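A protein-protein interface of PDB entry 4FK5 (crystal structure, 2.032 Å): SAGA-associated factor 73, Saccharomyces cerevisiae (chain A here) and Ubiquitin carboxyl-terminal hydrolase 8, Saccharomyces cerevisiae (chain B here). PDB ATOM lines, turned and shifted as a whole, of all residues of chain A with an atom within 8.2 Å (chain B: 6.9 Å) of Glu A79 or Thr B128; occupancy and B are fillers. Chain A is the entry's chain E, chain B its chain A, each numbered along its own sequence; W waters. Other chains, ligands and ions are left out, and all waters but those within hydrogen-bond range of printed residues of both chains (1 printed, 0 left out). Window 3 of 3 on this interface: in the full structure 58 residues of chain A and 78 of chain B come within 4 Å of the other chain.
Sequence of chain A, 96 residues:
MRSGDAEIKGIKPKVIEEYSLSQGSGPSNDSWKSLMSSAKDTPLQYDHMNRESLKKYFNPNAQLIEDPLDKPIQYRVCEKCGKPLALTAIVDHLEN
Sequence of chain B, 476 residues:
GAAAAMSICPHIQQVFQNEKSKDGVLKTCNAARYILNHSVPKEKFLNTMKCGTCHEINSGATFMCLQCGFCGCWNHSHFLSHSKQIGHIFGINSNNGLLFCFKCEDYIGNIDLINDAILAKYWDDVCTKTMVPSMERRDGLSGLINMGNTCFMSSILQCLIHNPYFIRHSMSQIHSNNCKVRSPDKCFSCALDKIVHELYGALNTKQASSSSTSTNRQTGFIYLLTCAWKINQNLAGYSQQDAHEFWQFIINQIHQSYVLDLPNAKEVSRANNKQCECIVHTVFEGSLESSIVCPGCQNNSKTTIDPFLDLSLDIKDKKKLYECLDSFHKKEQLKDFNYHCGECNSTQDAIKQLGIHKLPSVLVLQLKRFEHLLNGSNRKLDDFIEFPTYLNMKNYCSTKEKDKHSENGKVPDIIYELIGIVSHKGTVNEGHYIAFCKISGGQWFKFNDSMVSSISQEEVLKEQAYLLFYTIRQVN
The backbone carbonyl oxygen of Val B126 is in hydrogen-bond range of the side-chain hydroxyl of Thr B130, at 2.8 Å.
The backbone carbonyl oxygen (O) of Arg A76 sits at hydrogen-bond distance from the backbone NH (N) of Leu A85 (2.7 Å).
The side-chain amino group (NZ) of Lys B129 lies within salt-bridge range of the side-chain carboxylate (OD1) of Asp B125 (3.0 Å).
The side-chain sulfur (SG) of Cys A78 lies close to the backbone NH (N) of Lys A80, at 3.5 Å.
O of Asp B125 lies within hydrogen-bond range of OG1 of Thr B128.
O of Asp B124 lies close to OG1 of Thr B128 (3.4 Å).
Glu A79 touches four residues of chain B.
Leu A85 touches none of the printed residues of chain B.
Trp B123 touches none of the printed residues of chain A.
Of the printed residues of chain A, Val B126 touches Arg A76 (3.8 Å).
Thr B128 touches one residue of chain A.
Printed residues of chain A within 4 Å of Thr B130: Arg A76, Val A77 and Glu A79.
The nearest residue of chain A that does not touch Thr B128 is Arg A76 (6.0 Å).
The backbone carbonyl oxygen of Thr B128 lies close to the side-chain carboxylate of Glu A79 (3.0 Å).
O of Lys B129 sits at hydrogen-bond distance from N of Glu A79, at 3.1 Å.
The side-chain hydroxyl (OG1) of Thr B130 lies within hydrogen-bond range of the guanidinium group (NE) of Arg A76, 2.7 Å away.
The backbone carbonyl oxygen of Met B131 is in hydrogen-bond range of the backbone NH of Val A77 (2.7 Å).
Among the printed residues, pairs that only touch across the chains: Val A77 with Thr B130, Arg A76 with Met B131, Leu A94 with Lys B129, Glu A79 with Met B131, Leu A94 with Asp B125, Arg A76 with Val B132, Arg A76 with Val B126, Glu A79 with Thr B130 and Cys A78 with Lys B129.
Water W1 lies within hydrogen-bond range of O of Cys B127 (2.7 Å), O of Thr B130 (3.0 Å) and NH2 of Arg A76 (3.0 Å).
Hydrophobic or aromatic side chains of chain A within 4 Å of the printed part of chain B: Val A77 and Leu A94.
Of the 10 printed residues of chain B, 7 touch a printed residue of chain A.
Along chain B the printed residues that touch a printed residue of chain A span positions 125 to 132.
Among the printed residues, 13 pairs touch across the chains.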
ATOM      1  N   ARG A  76      23.337 -18.703   4.336  1.00  0.00           N
ATOM      2  CA  ARG A  76      24.585 -18.648   3.548  1.00  0.00           C
ATOM      3  C   ARG A  76      25.658 -19.402   4.314  1.00  0.00           C
ATOM      4  O   ARG A  76      25.513 -19.623   5.522  1.00  0.00           O
ATOM      5  CB  ARG A  76      24.987 -17.200   3.309  1.00  0.00           C
ATOM      6  CG  ARG A  76      24.044 -16.450   2.360  1.00  0.00           C
ATOM      7  CD  ARG A  76      24.474 -15.024   2.087  1.00  0.00           C
ATOM      8  NE  ARG A  76      25.659 -14.952   1.206  1.00  0.00           N
ATOM      9  CZ  ARG A  76      25.624 -14.785  -0.116  1.00  0.00           C
ATOM     10  NH1 ARG A  76      24.473 -14.666  -0.766  1.00  0.00           N
ATOM     11  NH2 ARG A  76      26.776 -14.764  -0.811  1.00  0.00           N
ATOM     12  N   VAL A  77      26.752 -19.782   3.616  1.00  0.00           N
ATOM     13  CA  VAL A  77      27.754 -20.679   4.166  1.00  0.00           C
ATOM     14  C   VAL A  77      29.096 -19.908   4.315  1.00  0.00           C
ATOM     15  O   VAL A  77      29.519 -19.211   3.408  1.00  0.00           O
ATOM     16  CB  VAL A  77      27.902 -21.908   3.269  1.00  0.00           C
ATOM     17  CG1 VAL A  77      29.153 -22.715   3.613  1.00  0.00           C
ATOM     18  CG2 VAL A  77      26.668 -22.781   3.384  1.00  0.00           C
ATOM     19  N   CYS A  78      29.659 -19.930   5.511  1.00  0.00           N
ATOM     20  CA  CYS A  78      30.874 -19.236   5.784  1.00  0.00           C
ATOM     21  C   CYS A  78      31.992 -19.841   4.920  1.00  0.00           C
ATOM     22  O   CYS A  78      32.196 -21.050   4.905  1.00  0.00           O
ATOM     23  CB  CYS A  78      31.256 -19.343   7.263  1.00  0.00           C
ATOM     24  SG  CYS A  78      32.902 -18.533   7.728  1.00  0.00           S
ATOM     25  N   GLU A  79      32.689 -18.994   4.211  1.00  0.00           N
ATOM     26  CA  GLU A  79      33.797 -19.453   3.360  1.00  0.00           C
ATOM     27  C   GLU A  79      35.058 -19.919   4.127  1.00  0.00           C
ATOM     28  O   GLU A  79      35.759 -20.779   3.661  1.00  0.00           O
ATOM     29  CB  GLU A  79      34.119 -18.403   2.314  1.00  0.00           C
ATOM     30  CG  GLU A  79      33.056 -18.421   1.222  1.00  0.00           C
ATOM     31  CD  GLU A  79      33.277 -17.397   0.151  1.00  0.00           C
ATOM     32  OE1 GLU A  79      34.259 -16.623   0.258  1.00  0.00           O
ATOM     33  OE2 GLU A  79      32.465 -17.364  -0.803  1.00  0.00           O
ATOM     34  N   LYS A  80      35.254 -19.426   5.336  1.00  0.00           N
ATOM     35  CA  LYS A  80      36.356 -19.905   6.224  1.00  0.00           C
ATOM     36  C   LYS A  80      36.100 -21.317   6.763  1.00  0.00           C
ATOM     37  O   LYS A  80      36.884 -22.229   6.517  1.00  0.00           O
ATOM     38  CB  LYS A  80      36.486 -18.963   7.411  1.00  0.00           C
ATOM     39  CG  LYS A  80      37.914 -18.642   7.817  1.00  0.00           C
ATOM     40  CD  LYS A  80      37.922 -17.501   8.837  1.00  0.00           C
ATOM     41  CE  LYS A  80      37.670 -18.001  10.276  1.00  0.00           C
ATOM     42  NZ  LYS A  80      37.048 -16.949  11.160  1.00  0.00           N
ATOM     43  N   CYS A  81      34.993 -21.476   7.518  1.00  0.00           N
ATOM     44  CA  CYS A  81      34.729 -22.671   8.313  1.00  0.00           C
ATOM     45  C   CYS A  81      33.575 -23.537   7.729  1.00  0.00           C
ATOM     46  O   CYS A  81      33.390 -24.685   8.114  1.00  0.00           O
ATOM     47  CB  CYS A  81      34.449 -22.292   9.797  1.00  0.00           C
ATOM     48  SG  CYS A  81      32.908 -21.362  10.082  1.00  0.00           S
ATOM     49  N   GLY A  82      32.903 -23.032   6.713  1.00  0.00           N
ATOM     50  CA  GLY A  82      31.890 -23.834   6.013  1.00  0.00           C
ATOM     51  C   GLY A  82      30.593 -24.009   6.821  1.00  0.00           C
ATOM     52  O   GLY A  82      29.756 -24.843   6.477  1.00  0.00           O
ATOM     53  N   LYS A  83      30.441 -23.244   7.902  1.00  0.00           N
ATOM     54  CA  LYS A  83      29.190 -23.283   8.729  1.00  0.00           C
ATOM     55  C   LYS A  83      27.984 -22.678   7.996  1.00  0.00           C
ATOM     56  O   LYS A  83      28.102 -21.648   7.330  1.00  0.00           O
ATOM     57  CB  LYS A  83      29.381 -22.547  10.038  1.00  0.00           C
ATOM     58  CG  LYS A  83      29.795 -23.451  11.195  1.00  0.00           C
ATOM     59  CD  LYS A  83      29.915 -22.684  12.527  1.00  0.00           C
ATOM     60  CE  LYS A  83      30.540 -23.585  13.587  1.00  0.00           C
ATOM     61  NZ  LYS A  83      30.675 -22.937  14.928  1.00  0.00           N
ATOM     62  N   LEU A  85      24.893 -20.405   8.026  1.00  0.00           N
ATOM     63  CA  LEU A  85      24.519 -19.278   8.833  1.00  0.00           C
ATOM     64  C   LEU A  85      23.196 -18.699   8.453  1.00  0.00           C
ATOM     65  O   LEU A  85      22.955 -18.350   7.279  1.00  0.00           O
ATOM     66  CB  LEU A  85      25.575 -18.188   8.724  1.00  0.00           C
ATOM     67  CG  LEU A  85      27.009 -18.577   9.048  1.00  0.00           C
ATOM     68  CD1 LEU A  85      27.937 -17.451   8.589  1.00  0.00           C
ATOM     69  CD2 LEU A  85      27.212 -18.930  10.551  1.00  0.00           C
ATOM     70  N   HIS A  93      29.094 -13.385  12.938  1.00  0.00           N
ATOM     71  CA  HIS A  93      30.023 -14.514  12.784  1.00  0.00           C
ATOM     72  C   HIS A  93      31.304 -14.031  12.167  1.00  0.00           C
ATOM     73  O   HIS A  93      32.383 -14.481  12.531  1.00  0.00           O
ATOM     74  CB  HIS A  93      29.420 -15.627  11.928  1.00  0.00           C
ATOM     75  CG  HIS A  93      30.395 -16.758  11.620  1.00  0.00           C
ATOM     76  ND1 HIS A  93      30.604 -17.800  12.473  1.00  0.00           N
ATOM     77  CD2 HIS A  93      31.215 -16.993  10.492  1.00  0.00           C
ATOM     78  CE1 HIS A  93      31.530 -18.652  11.942  1.00  0.00           C
ATOM     79  NE2 HIS A  93      31.938 -18.139  10.741  1.00  0.00           N
ATOM     80  N   LEU A  94      31.177 -13.122  11.208  1.00  0.00           N
ATOM     81  CA  LEU A  94      32.325 -12.589  10.460  1.00  0.00           C
ATOM     82  C   LEU A  94      33.263 -11.706  11.358  1.00  0.00           C
ATOM     83  O   LEU A  94      33.481 -10.516  11.060  1.00  0.00           O
ATOM     84  CB  LEU A  94      31.819 -11.775   9.252  1.00  0.00           C
ATOM     85  CG  LEU A  94      31.054 -12.556   8.169  1.00  0.00           C
ATOM     86  CD1 LEU A  94      30.617 -11.628   7.034  1.00  0.00           C
ATOM     87  CD2 LEU A  94      31.864 -13.741   7.618  1.00  0.00           C
ATOM     88  N   TRP B 123      26.320  -5.577   3.000  1.00  0.00           N
ATOM     89  CA  TRP B 123      26.255  -6.481   1.892  1.00  0.00           C
ATOM     90  C   TRP B 123      27.601  -6.827   1.272  1.00  0.00           C
ATOM     91  O   TRP B 123      27.775  -7.927   0.765  1.00  0.00           O
ATOM     92  CB  TRP B 123      25.341  -5.960   0.820  1.00  0.00           C
ATOM     93  CG  TRP B 123      24.990  -7.036  -0.142  1.00  0.00           C
ATOM     94  CD1 TRP B 123      25.311  -7.100  -1.480  1.00  0.00           C
ATOM     95  CD2 TRP B 123      24.298  -8.295   0.156  1.00  0.00           C
ATOM     96  NE1 TRP B 123      24.854  -8.268  -2.027  1.00  0.00           N
ATOM     97  CE2 TRP B 123      24.246  -9.032  -1.080  1.00  0.00           C
ATOM     98  CE3 TRP B 123      23.730  -8.843   1.294  1.00  0.00           C
ATOM     99  CZ2 TRP B 123      23.644 -10.286  -1.177  1.00  0.00           C
ATOM    100  CZ3 TRP B 123      23.111 -10.109   1.200  1.00  0.00           C
ATOM    101  CH2 TRP B 123      23.086 -10.820  -0.017  1.00  0.00           C
ATOM    102  N   ASP B 124      28.553  -5.905   1.269  1.00  0.00           N
ATOM    103  CA  ASP B 124      29.899  -6.240   0.684  1.00  0.00           C
ATOM    104  C   ASP B 124      30.623  -7.306   1.497  1.00  0.00           C
ATOM    105  O   ASP B 124      31.200  -8.243   0.945  1.00  0.00           O
ATOM    106  CB  ASP B 124      30.751  -4.999   0.574  1.00  0.00           C
ATOM    107  CG  ASP B 124      30.232  -4.049  -0.464  1.00  0.00           C
ATOM    108  OD1 ASP B 124      29.604  -4.528  -1.451  1.00  0.00           O
ATOM    109  OD2 ASP B 124      30.429  -2.831  -0.302  1.00  0.00           O
ATOM    110  N   ASP B 125      30.587  -7.131   2.812  1.00  0.00           N
ATOM    111  CA  ASP B 125      31.124  -8.075   3.780  1.00  0.00           C
ATOM    112  C   ASP B 125      30.412  -9.446   3.671  1.00  0.00           C
ATOM    113  O   ASP B 125      31.040 -10.483   3.573  1.00  0.00           O
ATOM    114  CB  ASP B 125      30.878  -7.499   5.187  1.00  0.00           C
ATOM    115  CG  ASP B 125      32.111  -7.577   6.106  1.00  0.00           C
ATOM    116  OD1 ASP B 125      32.804  -8.630   6.122  1.00  0.00           O
ATOM    117  OD2 ASP B 125      32.359  -6.575   6.835  1.00  0.00           O
ATOM    118  N   VAL B 126      29.076  -9.428   3.686  1.00  0.00           N
ATOM    119  CA  VAL B 126      28.333 -10.663   3.509  1.00  0.00           C
ATOM    120  C   VAL B 126      28.737 -11.370   2.196  1.00  0.00           C
ATOM    121  O   VAL B 126      29.019 -12.567   2.201  1.00  0.00           O
ATOM    122  CB  VAL B 126      26.784 -10.416   3.551  1.00  0.00           C
ATOM    123  CG1 VAL B 126      26.045 -11.645   3.049  1.00  0.00           C
ATOM    124  CG2 VAL B 126      26.348 -10.030   4.957  1.00  0.00           C
ATOM    125  N   CYS B 127      28.770 -10.640   1.092  1.00  0.00           N
ATOM    126  CA  CYS B 127      29.068 -11.238  -0.208  1.00  0.00           C
ATOM    127  C   CYS B 127      30.471 -11.847  -0.298  1.00  0.00           C
ATOM    128  O   CYS B 127      30.668 -12.881  -0.902  1.00  0.00           O
ATOM    129  CB  CYS B 127      28.896 -10.207  -1.325  1.00  0.00           C
ATOM    130  SG  CYS B 127      27.233 -10.199  -2.015  1.00  0.00           S
ATOM    131  N   THR B 128      31.441 -11.217   0.313  1.00  0.00           N
ATOM    132  CA  THR B 128      32.808 -11.688   0.153  1.00  0.00           C
ATOM    133  C   THR B 128      33.039 -12.862   1.084  1.00  0.00           C
ATOM    134  O   THR B 128      33.832 -13.743   0.795  1.00  0.00           O
ATOM    135  CB  THR B 128      33.826 -10.575   0.424  1.00  0.00           C
ATOM    136  OG1 THR B 128      33.773 -10.215   1.812  1.00  0.00           O
ATOM    137  CG2 THR B 128      33.528  -9.314  -0.489  1.00  0.00           C
ATOM    138  N   LYS B 129      32.315 -12.904   2.181  1.00  0.00           N
ATOM    139  CA  LYS B 129      32.693 -13.809   3.247  1.00  0.00           C
ATOM    140  C   LYS B 129      31.794 -14.996   3.431  1.00  0.00           C
ATOM    141  O   LYS B 129      32.130 -15.932   4.182  1.00  0.00           O
ATOM    142  CB  LYS B 129      32.869 -13.032   4.520  1.00  0.00           C
ATOM    143  CG  LYS B 129      34.223 -12.318   4.492  1.00  0.00           C
ATOM    144  CD  LYS B 129      34.231 -11.023   5.260  1.00  0.00           C
ATOM    145  CE  LYS B 129      35.661 -10.485   5.349  1.00  0.00           C
ATOM    146  NZ  LYS B 129      35.737  -9.407   6.344  1.00  0.00           N
ATOM    147  N   THR B 130      30.663 -14.987   2.706  1.00  0.00           N
ATOM    148  CA  THR B 130      29.804 -16.120   2.650  1.00  0.00           C
ATOM    149  C   THR B 130      29.353 -16.387   1.212  1.00  0.00           C
ATOM    150  O   THR B 130      29.291 -15.481   0.366  1.00  0.00           O
ATOM    151  CB  THR B 130      28.543 -15.919   3.568  1.00  0.00           C
ATOM    152  OG1 THR B 130      27.685 -14.922   3.015  1.00  0.00           O
ATOM    153  CG2 THR B 130      28.943 -15.527   5.003  1.00  0.00           C
ATOM    154  N   MET B 131      28.973 -17.616   0.965  1.00  0.00           N
ATOM    155  CA  MET B 131      28.466 -18.022  -0.314  1.00  0.00           C
ATOM    156  C   MET B 131      27.066 -18.666  -0.173  1.00  0.00           C
ATOM    157  O   MET B 131      26.640 -19.126   0.975  1.00  0.00           O
ATOM    158  CB  MET B 131      29.409 -19.039  -0.927  1.00  0.00           C
ATOM    159  CG  MET B 131      29.637 -20.260  -0.062  1.00  0.00           C
ATOM    160  SD  MET B 131      30.846 -21.416  -0.808  1.00  0.00           S
ATOM    161  CE  MET B 131      31.677 -22.013   0.685  1.00  0.00           C
ATOM    162  N   VAL B 132      26.347 -18.723  -1.287  1.00  0.00           N
ATOM    163  CA  VAL B 132      25.034 -19.441  -1.308  1.00  0.00           C
ATOM    164  C   VAL B 132      25.254 -20.916  -1.052  1.00  0.00           C
ATOM    165  O   VAL B 132      26.362 -21.424  -1.245  1.00  0.00           O
ATOM    166  CB  VAL B 132      24.259 -19.235  -2.638  1.00  0.00           C
ATOM    167  CG1 VAL B 132      24.086 -17.729  -2.925  1.00  0.00           C
ATOM    168  CG2 VAL B 132      24.971 -19.963  -3.804  1.00  0.00           C
HETATM  169  O   HOH W   1      29.284 -14.595  -2.517  1.00  0.00           O
